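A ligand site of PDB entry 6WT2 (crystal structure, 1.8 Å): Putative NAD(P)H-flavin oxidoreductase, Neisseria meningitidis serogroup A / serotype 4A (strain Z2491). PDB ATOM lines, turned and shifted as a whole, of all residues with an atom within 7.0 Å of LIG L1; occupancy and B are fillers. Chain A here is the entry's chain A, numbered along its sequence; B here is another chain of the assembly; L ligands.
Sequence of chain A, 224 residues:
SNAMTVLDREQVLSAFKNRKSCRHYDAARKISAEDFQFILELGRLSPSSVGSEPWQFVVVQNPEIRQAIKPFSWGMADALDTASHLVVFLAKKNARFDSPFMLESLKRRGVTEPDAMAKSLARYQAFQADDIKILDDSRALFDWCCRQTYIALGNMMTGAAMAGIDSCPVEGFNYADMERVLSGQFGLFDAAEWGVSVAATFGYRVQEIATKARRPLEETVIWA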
ATOM      1  N   SER A  48       6.222  26.712  14.978  1.00  0.00           N
ATOM      2  CA  SER A  48       5.051  26.016  14.476  1.00  0.00           C
ATOM      3  C   SER A  48       4.878  26.368  13.016  1.00  0.00           C
ATOM      4  O   SER A  48       5.245  27.464  12.577  1.00  0.00           O
ATOM      5  CB  SER A  48       3.789  26.377  15.266  1.00  0.00           C
ATOM      6  OG  SER A  48       3.598  27.774  15.280  1.00  0.00           O
ATOM      7  N   SER A  49       4.267  25.444  12.272  1.00  0.00           N
ATOM      8  CA  SER A  49       3.960  25.679  10.874  1.00  0.00           C
ATOM      9  C   SER A  49       3.158  26.967  10.730  1.00  0.00           C
ATOM     10  O   SER A  49       2.195  27.194  11.466  1.00  0.00           O
ATOM     11  CB  SER A  49       3.176  24.497  10.302  1.00  0.00           C
ATOM     12  OG  SER A  49       2.929  24.666   8.920  1.00  0.00           O
ATOM     13  N   VAL A  50       3.585  27.829   9.796  1.00  0.00           N
ATOM     14  CA  VAL A  50       3.040  29.156   9.492  1.00  0.00           C
ATOM     15  C   VAL A  50       2.830  29.993  10.735  1.00  0.00           C
ATOM     16  O   VAL A  50       2.035  30.938  10.723  1.00  0.00           O
ATOM     17  CB  VAL A  50       1.744  29.082   8.647  1.00  0.00           C
ATOM     18  CG1 VAL A  50       1.931  28.197   7.437  1.00  0.00           C
ATOM     19  CG2 VAL A  50       0.517  28.660   9.473  1.00  0.00           C
ATOM     20  N   GLY A  51       3.588  29.732  11.788  1.00  0.00           N
ATOM     21  CA  GLY A  51       3.425  30.505  13.006  1.00  0.00           C
ATOM     22  C   GLY A  51       2.044  30.364  13.617  1.00  0.00           C
ATOM     23  O   GLY A  51       1.563  31.294  14.281  1.00  0.00           O
ATOM     24  N   SER A  52       1.405  29.201  13.434  1.00  0.00           N
ATOM     25  CA  SER A  52       0.031  29.029  13.892  1.00  0.00           C
ATOM     26  C   SER A  52      -0.073  28.936  15.417  1.00  0.00           C
ATOM     27  O   SER A  52      -1.100  29.339  15.978  1.00  0.00           O
ATOM     28  CB  SER A  52      -0.559  27.771  13.249  1.00  0.00           C
ATOM     29  OG  SER A  52       0.283  26.657  13.524  1.00  0.00           O
ATOM     30  N   ARG A 109       2.197  37.378  12.489  1.00  0.00           N
ATOM     31  CA  ARG A 109       3.409  37.352  11.663  1.00  0.00           C
ATOM     32  C   ARG A 109       3.733  38.703  11.057  1.00  0.00           C
ATOM     33  O   ARG A 109       4.751  38.826  10.372  1.00  0.00           O
ATOM     34  CB  ARG A 109       3.266  36.341  10.532  1.00  0.00           C
ATOM     35  CG  ARG A 109       2.952  34.937  10.977  1.00  0.00           C
ATOM     36  CD  ARG A 109       3.074  33.966   9.815  1.00  0.00           C
ATOM     37  NE  ARG A 109       4.468  33.754   9.438  1.00  0.00           N
ATOM     38  CZ  ARG A 109       4.866  32.866   8.524  1.00  0.00           C
ATOM     39  NH1 ARG A 109       3.985  32.110   7.884  1.00  0.00           N
ATOM     40  NH2 ARG A 109       6.160  32.732   8.248  1.00  0.00           N
ATOM     41  N   ARG A 123      -1.822  31.331  -0.445  1.00  0.00           N
ATOM     42  CA  ARG A 123      -0.734  30.366  -0.337  1.00  0.00           C
ATOM     43  C   ARG A 123      -1.021  29.310   0.726  1.00  0.00           C
ATOM     44  O   ARG A 123      -0.760  28.121   0.519  1.00  0.00           O
ATOM     45  CB  ARG A 123       0.586  31.068  -0.043  1.00  0.00           C
ATOM     46  CG  ARG A 123       1.113  31.907  -1.206  1.00  0.00           C
ATOM     47  CD  ARG A 123       2.558  32.342  -0.968  1.00  0.00           C
ATOM     48  NE  ARG A 123       2.661  33.379   0.043  1.00  0.00           N
ATOM     49  CZ  ARG A 123       2.528  34.678  -0.211  1.00  0.00           C
ATOM     50  NH1 ARG A 123       2.274  35.081  -1.453  1.00  0.00           N
ATOM     51  NH2 ARG A 123       2.628  35.579   0.767  1.00  0.00           N
ATOM     52  N   TYR A 124      -1.563  29.733   1.883  1.00  0.00           N
ATOM     53  CA  TYR A 124      -1.944  28.759   2.912  1.00  0.00           C
ATOM     54  C   TYR A 124      -2.947  27.753   2.376  1.00  0.00           C
ATOM     55  O   TYR A 124      -2.879  26.570   2.688  1.00  0.00           O
ATOM     56  CB  TYR A 124      -2.537  29.455   4.128  1.00  0.00           C
ATOM     57  CG  TYR A 124      -1.604  30.284   4.998  1.00  0.00           C
ATOM     58  CD1 TYR A 124      -0.266  30.437   4.698  1.00  0.00           C
ATOM     59  CD2 TYR A 124      -2.092  30.888   6.156  1.00  0.00           C
ATOM     60  CE1 TYR A 124       0.576  31.201   5.520  1.00  0.00           C
ATOM     61  CE2 TYR A 124      -1.281  31.640   6.975  1.00  0.00           C
ATOM     62  CZ  TYR A 124       0.057  31.797   6.651  1.00  0.00           C
ATOM     63  OH  TYR A 124       0.849  32.560   7.493  1.00  0.00           O
ATOM     64  N   PHE A 127      -1.197  25.267   0.140  1.00  0.00           N
ATOM     65  CA  PHE A 127      -0.414  24.390   1.010  1.00  0.00           C
ATOM     66  C   PHE A 127      -1.298  23.321   1.632  1.00  0.00           C
ATOM     67  O   PHE A 127      -1.008  22.118   1.555  1.00  0.00           O
ATOM     68  CB  PHE A 127       0.278  25.216   2.091  1.00  0.00           C
ATOM     69  CG  PHE A 127       0.837  24.390   3.226  1.00  0.00           C
ATOM     70  CD1 PHE A 127       1.904  23.539   3.009  1.00  0.00           C
ATOM     71  CD2 PHE A 127       0.300  24.467   4.500  1.00  0.00           C
ATOM     72  CE1 PHE A 127       2.419  22.755   4.039  1.00  0.00           C
ATOM     73  CE2 PHE A 127       0.809  23.689   5.534  1.00  0.00           C
ATOM     74  CZ  PHE A 127       1.874  22.829   5.307  1.00  0.00           C
ATOM     75  N   ASP A 131      -0.508  20.431  -1.057  1.00  0.00           N
ATOM     76  CA  ASP A 131       0.829  19.965  -0.710  1.00  0.00           C
ATOM     77  C   ASP A 131       0.798  18.931   0.413  1.00  0.00           C
ATOM     78  O   ASP A 131       1.248  17.794   0.229  1.00  0.00           O
ATOM     79  CB  ASP A 131       1.725  21.144  -0.318  1.00  0.00           C
ATOM     80  CG  ASP A 131       2.053  22.037  -1.488  1.00  0.00           C
ATOM     81  OD1 ASP A 131       2.197  21.515  -2.622  1.00  0.00           O
ATOM     82  OD2 ASP A 131       2.151  23.269  -1.282  1.00  0.00           O
ATOM     83  N   TRP A 144      -2.535  17.567  11.955  1.00  0.00           N
ATOM     84  CA  TRP A 144      -1.554  18.594  11.600  1.00  0.00           C
ATOM     85  C   TRP A 144      -1.210  19.477  12.793  1.00  0.00           C
ATOM     86  O   TRP A 144      -0.032  19.696  13.117  1.00  0.00           O
ATOM     87  CB  TRP A 144      -2.075  19.430  10.439  1.00  0.00           C
ATOM     88  CG  TRP A 144      -1.160  20.541  10.001  1.00  0.00           C
ATOM     89  CD1 TRP A 144       0.144  20.429   9.610  1.00  0.00           C
ATOM     90  CD2 TRP A 144      -1.481  21.942   9.914  1.00  0.00           C
ATOM     91  NE1 TRP A 144       0.661  21.677   9.284  1.00  0.00           N
ATOM     92  CE2 TRP A 144      -0.327  22.614   9.470  1.00  0.00           C
ATOM     93  CE3 TRP A 144      -2.640  22.675  10.186  1.00  0.00           C
ATOM     94  CZ2 TRP A 144      -0.295  23.992   9.277  1.00  0.00           C
ATOM     95  CZ3 TRP A 144      -2.609  24.047  10.000  1.00  0.00           C
ATOM     96  CH2 TRP A 144      -1.445  24.696   9.536  1.00  0.00           C
ATOM     97  N   SER B  21      13.798  30.712  12.674  1.00  0.00           N
ATOM     98  CA  SER B  21      13.699  30.091  11.352  1.00  0.00           C
ATOM     99  C   SER B  21      14.516  30.892  10.324  1.00  0.00           C
ATOM    100  O   SER B  21      14.278  32.080  10.101  1.00  0.00           O
ATOM    101  CB  SER B  21      12.250  29.970  10.899  1.00  0.00           C
ATOM    102  OG  SER B  21      11.597  28.941  11.609  1.00  0.00           O
ATOM    103  N   ARG B  23      15.722  31.304   6.418  1.00  0.00           N
ATOM    104  CA  ARG B  23      15.438  30.939   5.034  1.00  0.00           C
ATOM    105  C   ARG B  23      16.604  31.189   4.090  1.00  0.00           C
ATOM    106  O   ARG B  23      16.559  30.732   2.947  1.00  0.00           O
ATOM    107  CB  ARG B  23      14.213  31.686   4.513  1.00  0.00           C
ATOM    108  CG  ARG B  23      12.899  31.123   5.010  1.00  0.00           C
ATOM    109  CD  ARG B  23      12.548  31.675   6.377  1.00  0.00           C
ATOM    110  NE  ARG B  23      11.290  31.142   6.883  1.00  0.00           N
ATOM    111  CZ  ARG B  23      10.617  31.683   7.896  1.00  0.00           C
ATOM    112  NH1 ARG B  23      11.070  32.784   8.492  1.00  0.00           N
ATOM    113  NH2 ARG B  23       9.479  31.147   8.292  1.00  0.00           N
ATOM    114  N   TRP B  74       8.510  24.848  -2.527  1.00  0.00           N
ATOM    115  CA  TRP B  74       8.547  26.313  -2.483  1.00  0.00           C
ATOM    116  C   TRP B  74       8.888  26.838  -1.090  1.00  0.00           C
ATOM    117  O   TRP B  74       9.481  27.912  -0.971  1.00  0.00           O
ATOM    118  CB  TRP B  74       7.211  26.878  -2.971  1.00  0.00           C
ATOM    119  CG  TRP B  74       6.021  26.270  -2.290  1.00  0.00           C
ATOM    120  CD1 TRP B  74       5.523  25.006  -2.478  1.00  0.00           C
ATOM    121  CD2 TRP B  74       5.182  26.895  -1.320  1.00  0.00           C
ATOM    122  NE1 TRP B  74       4.417  24.822  -1.684  1.00  0.00           N
ATOM    123  CE2 TRP B  74       4.190  25.964  -0.959  1.00  0.00           C
ATOM    124  CE3 TRP B  74       5.164  28.169  -0.728  1.00  0.00           C
ATOM    125  CZ2 TRP B  74       3.197  26.249  -0.032  1.00  0.00           C
ATOM    126  CZ3 TRP B  74       4.163  28.451   0.194  1.00  0.00           C
ATOM    127  CH2 TRP B  74       3.202  27.499   0.540  1.00  0.00           C
ATOM    128  N   GLY B  75       8.565  26.071  -0.049  1.00  0.00           N
ATOM    129  CA  GLY B  75       8.855  26.473   1.316  1.00  0.00           C
ATOM    130  C   GLY B  75      10.332  26.597   1.637  1.00  0.00           C
ATOM    131  O   GLY B  75      10.684  27.257   2.617  1.00  0.00           O
ATOM    132  N   MET B  76      11.206  25.955   0.851  1.00  0.00           N
ATOM    133  CA  MET B  76      12.636  26.101   1.088  1.00  0.00           C
ATOM    134  C   MET B  76      13.423  26.304  -0.212  1.00  0.00           C
ATOM    135  O   MET B  76      14.578  25.897  -0.296  1.00  0.00           O
ATOM    136  CB  MET B  76      13.167  24.862   1.824  1.00  0.00           C
ATOM    137  CG  MET B  76      12.756  23.562   1.168  1.00  0.00           C
ATOM    138  SD  MET B  76      13.756  22.016   1.850  1.00  0.00           S
ATOM    139  CE  MET B  76      12.726  20.644   0.959  1.00  0.00           C
ATOM    140  N   PRO B 169      12.538  24.660  10.147  1.00  0.00           N
ATOM    141  CA  PRO B 169      11.626  23.542   9.881  1.00  0.00           C
ATOM    142  C   PRO B 169      10.868  23.777   8.580  1.00  0.00           C
ATOM    143  O   PRO B 169      10.632  24.915   8.185  1.00  0.00           O
ATOM    144  CB  PRO B 169      10.673  23.544  11.087  1.00  0.00           C
ATOM    145  CG  PRO B 169      10.952  24.861  11.863  1.00  0.00           C
ATOM    146  CD  PRO B 169      11.959  25.663  11.060  1.00  0.00           C
ATOM    147  N   VAL B 170      10.500  22.680   7.903  1.00  0.00           N
ATOM    148  CA  VAL B 170       9.963  22.790   6.545  1.00  0.00           C
ATOM    149  C   VAL B 170       8.852  21.765   6.323  1.00  0.00           C
ATOM    150  O   VAL B 170       9.119  20.553   6.290  1.00  0.00           O
ATOM    151  CB  VAL B 170      11.046  22.620   5.463  1.00  0.00           C
ATOM    152  CG1 VAL B 170      10.416  22.738   4.084  1.00  0.00           C
ATOM    153  CG2 VAL B 170      12.152  23.670   5.610  1.00  0.00           C
ATOM    154  N   GLU B 171       7.621  22.249   6.121  1.00  0.00           N
ATOM    155  CA  GLU B 171       6.522  21.478   5.559  1.00  0.00           C
ATOM    156  C   GLU B 171       6.139  21.936   4.154  1.00  0.00           C
ATOM    157  O   GLU B 171       5.275  21.318   3.524  1.00  0.00           O
ATOM    158  CB  GLU B 171       5.270  21.560   6.447  1.00  0.00           C
ATOM    159  CG  GLU B 171       5.249  20.695   7.691  1.00  0.00           C
ATOM    160  CD  GLU B 171       4.103  21.087   8.641  1.00  0.00           C
ATOM    161  OE1 GLU B 171       3.371  22.049   8.306  1.00  0.00           O
ATOM    162  OE2 GLU B 171       3.928  20.463   9.702  1.00  0.00           O
ATOM    163  N   GLY B 172       6.726  23.020   3.654  1.00  0.00           N
ATOM    164  CA  GLY B 172       6.265  23.591   2.415  1.00  0.00           C
ATOM    165  C   GLY B 172       6.756  22.889   1.163  1.00  0.00           C
ATOM    166  O   GLY B 172       7.529  23.462   0.383  1.00  0.00           O
ATOM    167  N   PHE B 173       6.306  21.655   0.955  1.00  0.00           N
ATOM    168  CA  PHE B 173       6.600  20.937  -0.273  1.00  0.00           C
ATOM    169  C   PHE B 173       5.428  20.013  -0.575  1.00  0.00           C
ATOM    170  O   PHE B 173       4.624  19.703   0.299  1.00  0.00           O
ATOM    171  CB  PHE B 173       7.912  20.139  -0.164  1.00  0.00           C
ATOM    172  CG  PHE B 173       7.985  19.241   1.035  1.00  0.00           C
ATOM    173  CD1 PHE B 173       7.443  17.964   1.010  1.00  0.00           C
ATOM    174  CD2 PHE B 173       8.608  19.674   2.203  1.00  0.00           C
ATOM    175  CE1 PHE B 173       7.520  17.138   2.126  1.00  0.00           C
ATOM    176  CE2 PHE B 173       8.692  18.848   3.307  1.00  0.00           C
ATOM    177  CZ  PHE B 173       8.144  17.575   3.269  1.00  0.00           C
HETATM  178  N1  LIG L   1       5.097  27.340   3.666  1.00  0.00           N
HETATM  179  C1  LIG L   1       5.434  28.240   4.609  1.00  0.00           C
HETATM  180  C2  LIG L   1       5.276  27.936   5.952  1.00  0.00           C
HETATM  181  C3  LIG L   1       4.755  26.704   6.335  1.00  0.00           C
HETATM  182  C4  LIG L   1       4.396  25.803   5.346  1.00  0.00           C
HETATM  183  C5  LIG L   1       4.583  26.149   4.006  1.00  0.00           C
HETATM  184  C6  LIG L   1       5.656  28.954   7.001  1.00  0.00           C
HETATM  185  O1  LIG L   1       5.667  28.596   8.194  1.00  0.00           O
HETATM  186  O2  LIG L   1       5.937  30.124   6.647  1.00  0.00           O
HETATM  187  N1  LG2 L   2       9.146  28.202   7.215  1.00  0.00           N
HETATM  188  C1  LG2 L   2       9.344  28.285   5.875  1.00  0.00           C
HETATM  189  O1  LG2 L   2       9.839  29.336   5.426  1.00  0.00           O
HETATM  190  N2  LG2 L   2       8.895  27.356   5.012  1.00  0.00           N
HETATM  191  C2  LG2 L   2       8.305  26.219   5.434  1.00  0.00           C
HETATM  192  O2  LG2 L   2       7.983  25.304   4.645  1.00  0.00           O
HETATM  193  C3  LG2 L   2       8.119  26.028   6.881  1.00  0.00           C
HETATM  194  N3  LG2 L   2       7.391  25.002   7.358  1.00  0.00           N
HETATM  195  C4  LG2 L   2       7.322  24.797   8.685  1.00  0.00           C
HETATM  196  C5  LG2 L   2       6.913  23.544   9.148  1.00  0.00           C
HETATM  197  C6  LG2 L   2       6.818  23.351  10.509  1.00  0.00           C
HETATM  198  C7  LG2 L   2       6.379  22.004  11.032  1.00  0.00           C
HETATM  199  C8  LG2 L   2       7.349  24.377  11.450  1.00  0.00           C
HETATM  200  C9  LG2 L   2       7.372  24.148  12.936  1.00  0.00           C
HETATM  201  C10 LG2 L   2       7.764  25.624  10.982  1.00  0.00           C
HETATM  202  C11 LG2 L   2       7.858  25.810   9.628  1.00  0.00           C
HETATM  203  N4  LG2 L   2       8.370  27.037   9.141  1.00  0.00           N
HETATM  204  C12 LG2 L   2       8.503  27.163   7.750  1.00  0.00           C
HETATM  205  C13 LG2 L   2       8.879  28.065  10.053  1.00  0.00           C
HETATM  206  C14 LG2 L   2       7.721  28.860  10.690  1.00  0.00           C
HETATM  207  O3  LG2 L   2       7.201  29.809   9.748  1.00  0.00           O
HETATM  208  C15 LG2 L   2       8.276  29.595  11.900  1.00  0.00           C
HETATM  209  O4  LG2 L   2       8.649  28.619  12.876  1.00  0.00           O
HETATM  210  C16 LG2 L   2       7.261  30.549  12.530  1.00  0.00           C
HETATM  211  O5  LG2 L   2       6.883  31.494  11.524  1.00  0.00           O
HETATM  212  C17 LG2 L   2       7.877  31.265  13.717  1.00  0.00           C
HETATM  213  O6  LG2 L   2       9.140  31.819  13.330  1.00  0.00           O
HETATM  214  P1  LG2 L   2      10.447  31.466  14.199  1.00  0.00           P
HETATM  215  O7  LG2 L   2      10.098  31.863  15.599  1.00  0.00           O
HETATM  216  O8  LG2 L   2      11.557  32.232  13.545  1.00  0.00           O
HETATM  217  O9  LG2 L   2      10.573  29.957  13.985  1.00  0.00           O
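The side-chain carboxylate (OD2) of Asp 131 is in hydrogen-bond range of the indole nitrogen (NE1) of Trp 74 of chain B, at 2.8 Å.
O of Gly 172 of chain B is in hydrogen-bond range of N of Trp 74 of chain B, 3.4 Å away.
N of Gly 75 of chain B lies within hydrogen-bond range of O of Gly 172 of chain B (2.8 Å).
OG of Ser 49 sits at hydrogen-bond distance from OE1 of Glu 171 of chain B (2.7 Å).
OG of Ser 52 sits at hydrogen-bond distance from O of Ser 49, at 2.9 Å.
The guanidinium group of Arg 109 is in hydrogen-bond range of the side-chain hydroxyl of Tyr 124 (3.2 Å).
NH2 of Arg 109 sits at hydrogen-bond distance from O3 of LG2 L2 (3.4 Å).
The guanidinium group of Arg 23 of chain B sits at hydrogen-bond distance from an oxygen (O1) of LG2 L2.
An oxygen (O8) of LG2 L2 sits at hydrogen-bond distance from the backbone NH (N) of Ser 21 of chain B, 2.8 Å away.
NH1 of Arg 109 lies within salt-bridge range of O2 of LIG L1.
The backbone NH (N) of Gly 172 of chain B lies within hydrogen-bond range of an oxygen (O2) of LG2 L2 (2.8 Å).
A nitrogen (N2) of LG2 L2 is in hydrogen-bond range of the backbone carbonyl oxygen of Gly 75 of chain B (3.0 Å).
The side-chain hydroxyl (OG) of Ser 21 of chain B sits at hydrogen-bond distance from an oxygen (O9) of LG2 L2, at 2.8 Å.
The backbone NH of Glu 171 of chain B lies within hydrogen-bond range of a nitrogen (N3) of LG2 L2, at 3.0 Å.
An oxygen (O1) of LIG L1 is in hydrogen-bond range of the backbone NH of Val 50.
Merely in contact with LIG L1: Ser 49 (3.8 Å), Phe 127 (3.9 Å), Trp 74 of chain B (3.7 Å) and Gly 172 of chain B (3.5 Å).
Hydrophobic or aromatic side chains that line LIG L1: Val 50, Phe 127 and Trp 74 of chain B.
Of the 21 residues printed, 6 come within 4 Å of LIG L1.
O1 of LIG L1 is in hydrogen-bond range of O3 of LG2 L2, at 2.5 Å.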
